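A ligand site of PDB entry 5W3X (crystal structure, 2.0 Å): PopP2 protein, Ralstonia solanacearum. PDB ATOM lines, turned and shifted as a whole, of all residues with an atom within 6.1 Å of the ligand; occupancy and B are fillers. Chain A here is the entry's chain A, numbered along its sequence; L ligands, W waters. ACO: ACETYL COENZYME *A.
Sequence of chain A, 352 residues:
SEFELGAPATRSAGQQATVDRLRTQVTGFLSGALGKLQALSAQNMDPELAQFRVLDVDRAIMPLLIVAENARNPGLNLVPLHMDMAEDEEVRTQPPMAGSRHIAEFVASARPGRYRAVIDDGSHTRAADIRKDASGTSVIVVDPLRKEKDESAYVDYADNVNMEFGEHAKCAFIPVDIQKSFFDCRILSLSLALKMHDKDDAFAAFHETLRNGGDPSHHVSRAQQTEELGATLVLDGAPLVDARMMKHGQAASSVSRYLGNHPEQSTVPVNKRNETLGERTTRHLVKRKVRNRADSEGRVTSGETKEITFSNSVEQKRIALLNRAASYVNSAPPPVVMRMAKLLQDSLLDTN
The backbone NH (N) of Ser 253 lies within hydrogen-bond range of an oxygen (O8A) of the ligand (3.0 Å).
OG of Ser 253 lies within hydrogen-bond range of O7A of the ligand (2.7 Å).
O of Thr 309 sits at hydrogen-bond distance from O2B of the ligand (2.8 Å).
An oxygen (O4A) of the ligand sits at hydrogen-bond distance from the backbone NH of Ser 296, 3.3 Å away.
An oxygen (O4A) of the ligand is in hydrogen-bond range of the side-chain hydroxyl of Ser 296 (2.9 Å).
The backbone NH (N) of Ala 252 sits at hydrogen-bond distance from an oxygen (O8A) of the ligand (3.4 Å).
The backbone NH (N) of Lys 180 is in hydrogen-bond range of the side-chain amide oxygen (OE1) of Gln 250 (2.7 Å).
OD1 of Asp 295 sits at hydrogen-bond distance from N of Glu 297 (3.2 Å).
The backbone NH (N) of Ser 181 sits at hydrogen-bond distance from the side-chain amide oxygen (OE1) of Gln 250.
The side-chain carboxylate (OD2) of Asp 184 is in hydrogen-bond range of the side-chain hydroxyl (OG) of Ser 181 (2.6 Å).
CB of Lys 180 touches C4A of the ligand, at 3.4 Å.
Ser 181 touches the ligand.
Ala 251 touches the ligand.
CB of Asp 295 touches O4A of the ligand, 3.5 Å away.
Ile 308 touches the ligand (CD1 to C4A, 3.3 Å).
Phe 310 touches the ligand.
Water W11 bridges O5B of the ligand (2.6 Å) and NZ of Lys 306 (3.4 Å).
Water W5 lies within hydrogen-bond range of O8A of the ligand (2.6 Å), O of Thr 309 (2.8 Å) and N of Ala 252 (3.0 Å).
Water W4 bridges N7A of the ligand (2.7 Å) and NZ of Lys 306 (3.1 Å).
Water W6 lies within hydrogen-bond range of the guanidinium group of Arg 293 (2.9 Å), the backbone carbonyl oxygen of Arg 291 (2.9 Å) and a nitrogen (N6A) of the ligand (3.2 Å).
Water W2 bridges the side-chain carboxylate (OD1) of Asp 46 (2.8 Å) and a nitrogen (N6A) of the ligand (3.2 Å).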
ATOM      1  N   ASP A  46      11.267 -31.281 -36.115  1.00  0.00           N
ATOM      2  CA  ASP A  46      10.179 -30.688 -35.345  1.00  0.00           C
ATOM      3  C   ASP A  46       9.071 -30.221 -36.290  1.00  0.00           C
ATOM      4  O   ASP A  46       9.341 -29.530 -37.277  1.00  0.00           O
ATOM      5  CB  ASP A  46      10.694 -29.527 -34.524  1.00  0.00           C
ATOM      6  CG  ASP A  46       9.572 -28.786 -33.805  1.00  0.00           C
ATOM      7  OD1 ASP A  46       8.971 -29.368 -32.871  1.00  0.00           O
ATOM      8  OD2 ASP A  46       9.296 -27.617 -34.157  1.00  0.00           O
ATOM      9  N   LYS A 180       5.665 -30.973 -22.630  1.00  0.00           N
ATOM     10  CA  LYS A 180       6.554 -29.831 -22.702  1.00  0.00           C
ATOM     11  C   LYS A 180       6.314 -28.980 -23.952  1.00  0.00           C
ATOM     12  O   LYS A 180       6.671 -27.803 -23.967  1.00  0.00           O
ATOM     13  CB  LYS A 180       8.007 -30.296 -22.645  1.00  0.00           C
ATOM     14  CG  LYS A 180       8.381 -30.900 -21.305  1.00  0.00           C
ATOM     15  CD  LYS A 180       8.306 -29.862 -20.174  1.00  0.00           C
ATOM     16  CE  LYS A 180       8.684 -30.489 -18.825  1.00  0.00           C
ATOM     17  NZ  LYS A 180       8.663 -29.499 -17.701  1.00  0.00           N
ATOM     18  N   SER A 181       5.701 -29.563 -24.974  1.00  0.00           N
ATOM     19  CA  SER A 181       5.394 -28.835 -26.214  1.00  0.00           C
ATOM     20  C   SER A 181       4.093 -28.052 -26.143  1.00  0.00           C
ATOM     21  O   SER A 181       3.314 -28.191 -25.186  1.00  0.00           O
ATOM     22  CB  SER A 181       5.302 -29.812 -27.380  1.00  0.00           C
ATOM     23  OG  SER A 181       4.078 -30.512 -27.275  1.00  0.00           O
ATOM     24  N   PHE A 182       3.820 -27.258 -27.169  1.00  0.00           N
ATOM     25  CA  PHE A 182       2.589 -26.475 -27.194  1.00  0.00           C
ATOM     26  C   PHE A 182       1.405 -27.243 -27.803  1.00  0.00           C
ATOM     27  O   PHE A 182       0.270 -26.769 -27.728  1.00  0.00           O
ATOM     28  CB  PHE A 182       2.792 -25.153 -27.950  1.00  0.00           C
ATOM     29  CG  PHE A 182       2.884 -25.309 -29.461  1.00  0.00           C
ATOM     30  CD1 PHE A 182       1.744 -25.222 -30.247  1.00  0.00           C
ATOM     31  CD2 PHE A 182       4.104 -25.506 -30.084  1.00  0.00           C
ATOM     32  CE1 PHE A 182       1.826 -25.353 -31.633  1.00  0.00           C
ATOM     33  CE2 PHE A 182       4.184 -25.635 -31.456  1.00  0.00           C
ATOM     34  CZ  PHE A 182       3.042 -25.547 -32.228  1.00  0.00           C
ATOM     35  N   ASP A 184       1.037 -31.140 -27.895  1.00  0.00           N
ATOM     36  CA  ASP A 184       0.846 -32.574 -27.645  1.00  0.00           C
ATOM     37  C   ASP A 184      -0.266 -32.937 -26.640  1.00  0.00           C
ATOM     38  O   ASP A 184      -0.492 -34.109 -26.373  1.00  0.00           O
ATOM     39  CB  ASP A 184       2.181 -33.195 -27.179  1.00  0.00           C
ATOM     40  CG  ASP A 184       3.170 -33.362 -28.357  1.00  0.00           C
ATOM     41  OD1 ASP A 184       2.761 -33.916 -29.391  1.00  0.00           O
ATOM     42  OD2 ASP A 184       4.346 -32.954 -28.238  1.00  0.00           O
ATOM     43  N   GLN A 250       7.798 -35.957 -21.722  1.00  0.00           N
ATOM     44  CA  GLN A 250       8.708 -35.505 -22.777  1.00  0.00           C
ATOM     45  C   GLN A 250      10.089 -35.096 -22.262  1.00  0.00           C
ATOM     46  O   GLN A 250      11.102 -35.255 -22.954  1.00  0.00           O
ATOM     47  CB  GLN A 250       8.053 -34.344 -23.538  1.00  0.00           C
ATOM     48  CG  GLN A 250       6.759 -34.763 -24.246  1.00  0.00           C
ATOM     49  CD  GLN A 250       6.257 -33.707 -25.216  1.00  0.00           C
ATOM     50  OE1 GLN A 250       5.867 -32.613 -24.822  1.00  0.00           O
ATOM     51  NE2 GLN A 250       6.282 -34.036 -26.503  1.00  0.00           N
ATOM     52  N   ALA A 251      10.149 -34.593 -21.029  1.00  0.00           N
ATOM     53  CA  ALA A 251      11.484 -34.273 -20.470  1.00  0.00           C
ATOM     54  C   ALA A 251      11.974 -35.389 -19.554  1.00  0.00           C
ATOM     55  O   ALA A 251      11.306 -35.753 -18.597  1.00  0.00           O
ATOM     56  CB  ALA A 251      11.443 -32.959 -19.730  1.00  0.00           C
ATOM     57  N   ALA A 252      13.152 -35.924 -19.867  1.00  0.00           N
ATOM     58  CA  ALA A 252      13.812 -36.888 -18.982  1.00  0.00           C
ATOM     59  C   ALA A 252      13.844 -36.371 -17.531  1.00  0.00           C
ATOM     60  O   ALA A 252      13.651 -37.140 -16.595  1.00  0.00           O
ATOM     61  CB  ALA A 252      15.240 -37.171 -19.481  1.00  0.00           C
ATOM     62  N   SER A 253      14.044 -35.069 -17.363  1.00  0.00           N
ATOM     63  CA  SER A 253      14.146 -34.500 -16.007  1.00  0.00           C
ATOM     64  C   SER A 253      12.820 -34.647 -15.235  1.00  0.00           C
ATOM     65  O   SER A 253      12.838 -34.868 -14.026  1.00  0.00           O
ATOM     66  CB  SER A 253      14.570 -33.014 -16.065  1.00  0.00           C
ATOM     67  OG  SER A 253      13.595 -32.213 -16.713  1.00  0.00           O
ATOM     68  N   SER A 254      11.695 -34.565 -15.939  1.00  0.00           N
ATOM     69  CA  SER A 254      10.368 -34.750 -15.307  1.00  0.00           C
ATOM     70  C   SER A 254      10.155 -36.185 -14.837  1.00  0.00           C
ATOM     71  O   SER A 254       9.637 -36.456 -13.749  1.00  0.00           O
ATOM     72  CB  SER A 254       9.251 -34.355 -16.274  1.00  0.00           C
ATOM     73  OG  SER A 254       9.383 -33.008 -16.685  1.00  0.00           O
ATOM     74  N   VAL A 290      14.153 -27.083 -32.008  1.00  0.00           N
ATOM     75  CA  VAL A 290      12.779 -26.649 -31.861  1.00  0.00           C
ATOM     76  C   VAL A 290      12.816 -25.137 -31.764  1.00  0.00           C
ATOM     77  O   VAL A 290      13.884 -24.555 -31.552  1.00  0.00           O
ATOM     78  CB  VAL A 290      12.092 -27.265 -30.621  1.00  0.00           C
ATOM     79  CG1 VAL A 290      11.963 -28.761 -30.764  1.00  0.00           C
ATOM     80  CG2 VAL A 290      12.862 -26.890 -29.326  1.00  0.00           C
ATOM     81  N   ARG A 291      11.663 -24.487 -31.899  1.00  0.00           N
ATOM     82  CA  ARG A 291      11.591 -23.033 -31.728  1.00  0.00           C
ATOM     83  C   ARG A 291      12.075 -22.650 -30.338  1.00  0.00           C
ATOM     84  O   ARG A 291      11.738 -23.313 -29.351  1.00  0.00           O
ATOM     85  CB  ARG A 291      10.183 -22.519 -31.970  1.00  0.00           C
ATOM     86  CG  ARG A 291       9.914 -21.139 -31.378  1.00  0.00           C
ATOM     87  CD  ARG A 291       8.544 -20.625 -31.823  1.00  0.00           C
ATOM     88  NE  ARG A 291       8.427 -20.676 -33.280  1.00  0.00           N
ATOM     89  CZ  ARG A 291       8.833 -19.704 -34.094  1.00  0.00           C
ATOM     90  NH1 ARG A 291       9.378 -18.593 -33.586  1.00  0.00           N
ATOM     91  NH2 ARG A 291       8.702 -19.842 -35.399  1.00  0.00           N
ATOM     92  N   ARG A 293      11.983 -20.953 -27.023  1.00  0.00           N
ATOM     93  CA  ARG A 293      10.907 -20.418 -26.217  1.00  0.00           C
ATOM     94  C   ARG A 293      11.471 -20.126 -24.847  1.00  0.00           C
ATOM     95  O   ARG A 293      12.489 -20.701 -24.469  1.00  0.00           O
ATOM     96  CB  ARG A 293       9.723 -21.395 -26.111  1.00  0.00           C
ATOM     97  CG  ARG A 293       8.813 -21.393 -27.318  1.00  0.00           C
ATOM     98  CD  ARG A 293       7.567 -22.255 -27.098  1.00  0.00           C
ATOM     99  NE  ARG A 293       6.604 -22.015 -28.166  1.00  0.00           N
ATOM    100  CZ  ARG A 293       6.612 -22.679 -29.320  1.00  0.00           C
ATOM    101  NH1 ARG A 293       7.514 -23.635 -29.541  1.00  0.00           N
ATOM    102  NH2 ARG A 293       5.717 -22.386 -30.253  1.00  0.00           N
ATOM    103  N   ALA A 294      10.827 -19.216 -24.130  1.00  0.00           N
ATOM    104  CA  ALA A 294      11.212 -18.887 -22.766  1.00  0.00           C
ATOM    105  C   ALA A 294      11.133 -20.124 -21.869  1.00  0.00           C
ATOM    106  O   ALA A 294      10.329 -21.031 -22.110  1.00  0.00           O
ATOM    107  CB  ALA A 294      10.330 -17.782 -22.226  1.00  0.00           C
ATOM    108  N   ASP A 295      11.979 -20.154 -20.843  1.00  0.00           N
ATOM    109  CA  ASP A 295      11.985 -21.228 -19.847  1.00  0.00           C
ATOM    110  C   ASP A 295      11.049 -20.899 -18.678  1.00  0.00           C
ATOM    111  O   ASP A 295      10.229 -19.990 -18.777  1.00  0.00           O
ATOM    112  CB  ASP A 295      13.411 -21.511 -19.352  1.00  0.00           C
ATOM    113  CG  ASP A 295      14.098 -20.276 -18.812  1.00  0.00           C
ATOM    114  OD1 ASP A 295      13.416 -19.334 -18.350  1.00  0.00           O
ATOM    115  OD2 ASP A 295      15.351 -20.249 -18.834  1.00  0.00           O
ATOM    116  N   SER A 296      11.192 -21.646 -17.578  1.00  0.00           N
ATOM    117  CA  SER A 296      10.369 -21.462 -16.382  1.00  0.00           C
ATOM    118  C   SER A 296      10.303 -20.021 -15.869  1.00  0.00           C
ATOM    119  O   SER A 296       9.220 -19.527 -15.557  1.00  0.00           O
ATOM    120  CB  SER A 296      10.891 -22.358 -15.246  1.00  0.00           C
ATOM    121  OG  SER A 296      10.884 -23.723 -15.627  1.00  0.00           O
ATOM    122  N   GLU A 297      11.451 -19.355 -15.775  1.00  0.00           N
ATOM    123  CA  GLU A 297      11.475 -17.984 -15.261  1.00  0.00           C
ATOM    124  C   GLU A 297      11.390 -17.000 -16.426  1.00  0.00           C
ATOM    125  O   GLU A 297      11.688 -15.815 -16.293  1.00  0.00           O
ATOM    126  CB  GLU A 297      12.730 -17.728 -14.405  1.00  0.00           C
ATOM    127  CG  GLU A 297      12.649 -16.474 -13.514  1.00  0.00           C
ATOM    128  CD  GLU A 297      11.336 -16.384 -12.730  1.00  0.00           C
ATOM    129  OE1 GLU A 297      11.248 -16.997 -11.641  1.00  0.00           O
ATOM    130  OE2 GLU A 297      10.409 -15.680 -13.185  1.00  0.00           O
ATOM    131  N   LYS A 306      16.455 -23.539 -30.627  1.00  0.00           N
ATOM    132  CA  LYS A 306      17.353 -24.109 -29.613  1.00  0.00           C
ATOM    133  C   LYS A 306      17.372 -25.621 -29.838  1.00  0.00           C
ATOM    134  O   LYS A 306      16.411 -26.183 -30.373  1.00  0.00           O
ATOM    135  CB  LYS A 306      16.896 -23.789 -28.189  1.00  0.00           C
ATOM    136  CG  LYS A 306      15.547 -24.402 -27.825  1.00  0.00           C
ATOM    137  CD  LYS A 306      15.055 -23.983 -26.439  1.00  0.00           C
ATOM    138  CE  LYS A 306      13.608 -24.441 -26.224  1.00  0.00           C
ATOM    139  NZ  LYS A 306      13.035 -23.948 -24.938  1.00  0.00           N
ATOM    140  N   ILE A 308      17.358 -29.281 -28.115  1.00  0.00           N
ATOM    141  CA  ILE A 308      17.038 -29.898 -26.841  1.00  0.00           C
ATOM    142  C   ILE A 308      17.076 -31.405 -26.948  1.00  0.00           C
ATOM    143  O   ILE A 308      17.029 -31.966 -28.035  1.00  0.00           O
ATOM    144  CB  ILE A 308      15.652 -29.494 -26.333  1.00  0.00           C
ATOM    145  CG1 ILE A 308      14.601 -29.884 -27.363  1.00  0.00           C
ATOM    146  CG2 ILE A 308      15.609 -28.002 -26.052  1.00  0.00           C
ATOM    147  CD1 ILE A 308      13.167 -29.696 -26.876  1.00  0.00           C
ATOM    148  N   THR A 309      17.167 -32.051 -25.796  1.00  0.00           N
ATOM    149  CA  THR A 309      17.033 -33.489 -25.744  1.00  0.00           C
ATOM    150  C   THR A 309      15.728 -33.812 -25.044  1.00  0.00           C
ATOM    151  O   THR A 309      15.477 -33.325 -23.934  1.00  0.00           O
ATOM    152  CB  THR A 309      18.206 -34.160 -25.027  1.00  0.00           C
ATOM    153  OG1 THR A 309      19.412 -33.883 -25.746  1.00  0.00           O
ATOM    154  CG2 THR A 309      18.005 -35.662 -24.958  1.00  0.00           C
ATOM    155  N   PHE A 310      14.887 -34.610 -25.692  1.00  0.00           N
ATOM    156  CA  PHE A 310      13.613 -34.967 -25.076  1.00  0.00           C
ATOM    157  C   PHE A 310      13.167 -36.323 -25.591  1.00  0.00           C
ATOM    158  O   PHE A 310      13.735 -36.851 -26.556  1.00  0.00           O
ATOM    159  CB  PHE A 310      12.548 -33.904 -25.363  1.00  0.00           C
ATOM    160  CG  PHE A 310      12.074 -33.901 -26.792  1.00  0.00           C
ATOM    161  CD1 PHE A 310      12.801 -33.246 -27.770  1.00  0.00           C
ATOM    162  CD2 PHE A 310      10.923 -34.578 -27.153  1.00  0.00           C
ATOM    163  CE1 PHE A 310      12.359 -33.250 -29.099  1.00  0.00           C
ATOM    164  CE2 PHE A 310      10.490 -34.583 -28.480  1.00  0.00           C
ATOM    165  CZ  PHE A 310      11.218 -33.921 -29.452  1.00  0.00           C
ATOM    166  N   SER A 311      12.137 -36.861 -24.972  1.00  0.00           N
ATOM    167  CA  SER A 311      11.611 -38.160 -25.333  1.00  0.00           C
ATOM    168  C   SER A 311      10.599 -38.082 -26.472  1.00  0.00           C
ATOM    169  O   SER A 311       9.624 -37.324 -26.401  1.00  0.00           O
ATOM    170  CB  SER A 311      10.945 -38.803 -24.123  1.00  0.00           C
ATOM    171  OG  SER A 311      10.224 -39.963 -24.517  1.00  0.00           O
HETATM  172  N1A ACO L   1       9.245 -30.377 -26.948  1.00  0.00           N
HETATM  173  C2A ACO L   1       9.726 -31.359 -26.127  1.00  0.00           C
HETATM  174  N3A ACO L   1      10.456 -31.300 -25.000  1.00  0.00           N
HETATM  175  C4A ACO L   1      10.740 -29.996 -24.666  1.00  0.00           C
HETATM  176  C5A ACO L   1      10.317 -28.861 -25.422  1.00  0.00           C
HETATM  177  C6A ACO L   1       9.554 -29.110 -26.570  1.00  0.00           C
HETATM  178  N6A ACO L   1       9.108 -28.060 -27.349  1.00  0.00           N
HETATM  179  N7A ACO L   1      10.772 -27.670 -24.852  1.00  0.00           N
HETATM  180  C8A ACO L   1      11.459 -28.090 -23.774  1.00  0.00           C
HETATM  181  N9A ACO L   1      11.460 -29.484 -23.625  1.00  0.00           N
HETATM  182  C1B ACO L   1      12.127 -30.258 -22.579  1.00  0.00           C
HETATM  183  C2B ACO L   1      13.675 -29.957 -22.673  1.00  0.00           C
HETATM  184  O2B ACO L   1      14.306 -30.863 -23.487  1.00  0.00           O
HETATM  185  C3B ACO L   1      14.068 -30.191 -21.168  1.00  0.00           C
HETATM  186  O3B ACO L   1      14.286 -31.497 -20.977  1.00  0.00           O
HETATM  187  P3B ACO L   1      15.494 -31.886 -19.664  1.00  0.00           P
HETATM  188  O7A ACO L   1      14.956 -30.968 -18.620  1.00  0.00           O
HETATM  189  O8A ACO L   1      15.313 -33.384 -19.477  1.00  0.00           O
HETATM  190  O9A ACO L   1      16.732 -31.376 -20.367  1.00  0.00           O
HETATM  191  C4B ACO L   1      12.750 -29.740 -20.423  1.00  0.00           C
HETATM  192  O4B ACO L   1      11.641 -29.751 -21.360  1.00  0.00           O
HETATM  193  C5B ACO L   1      12.913 -28.355 -19.808  1.00  0.00           C
HETATM  194  O5B ACO L   1      13.350 -27.445 -20.797  1.00  0.00           O
HETATM  195  P1A ACO L   1      12.985 -25.957 -20.189  1.00  0.00           P
HETATM  196  O1A ACO L   1      14.202 -25.199 -19.711  1.00  0.00           O
HETATM  197  O2A ACO L   1      12.034 -25.312 -21.119  1.00  0.00           O
HETATM  198  O3A ACO L   1      11.952 -26.182 -18.854  1.00  0.00           O
HETATM  199  P2A ACO L   1      12.672 -25.770 -17.478  1.00  0.00           P
HETATM  200  O4A ACO L   1      13.110 -24.334 -17.385  1.00  0.00           O
HETATM  201  O5A ACO L   1      11.946 -26.467 -16.387  1.00  0.00           O
HETATM  202  O6A ACO L   1      14.192 -26.632 -17.417  1.00  0.00           O
HETATM  203  O   HOH W   1      18.010 -28.917 -19.721  1.00  0.00           O
HETATM  204  O   HOH W   2       7.987 -28.905 -30.275  1.00  0.00           O
HETATM  205  O   HOH W   3      15.576 -28.838 -16.702  1.00  0.00           O
HETATM  206  O   HOH W   4      10.139 -25.069 -25.352  1.00  0.00           O
HETATM  207  O   HOH W   5      15.299 -34.860 -21.622  1.00  0.00           O
HETATM  208  O   HOH W   6       9.677 -25.038 -28.289  1.00  0.00           O
HETATM  209  O   HOH W   7       8.490 -31.407 -29.266  1.00  0.00           O
HETATM  210  O   HOH W   8       6.443 -26.651 -28.354  1.00  0.00           O
HETATM  211  O   HOH W   9      17.417 -34.352 -18.073  1.00  0.00           O
HETATM  212  O   HOH W  10      19.151 -33.318 -19.433  1.00  0.00           O
HETATM  213  O   HOH W  11      14.491 -25.763 -22.407  1.00  0.00           O
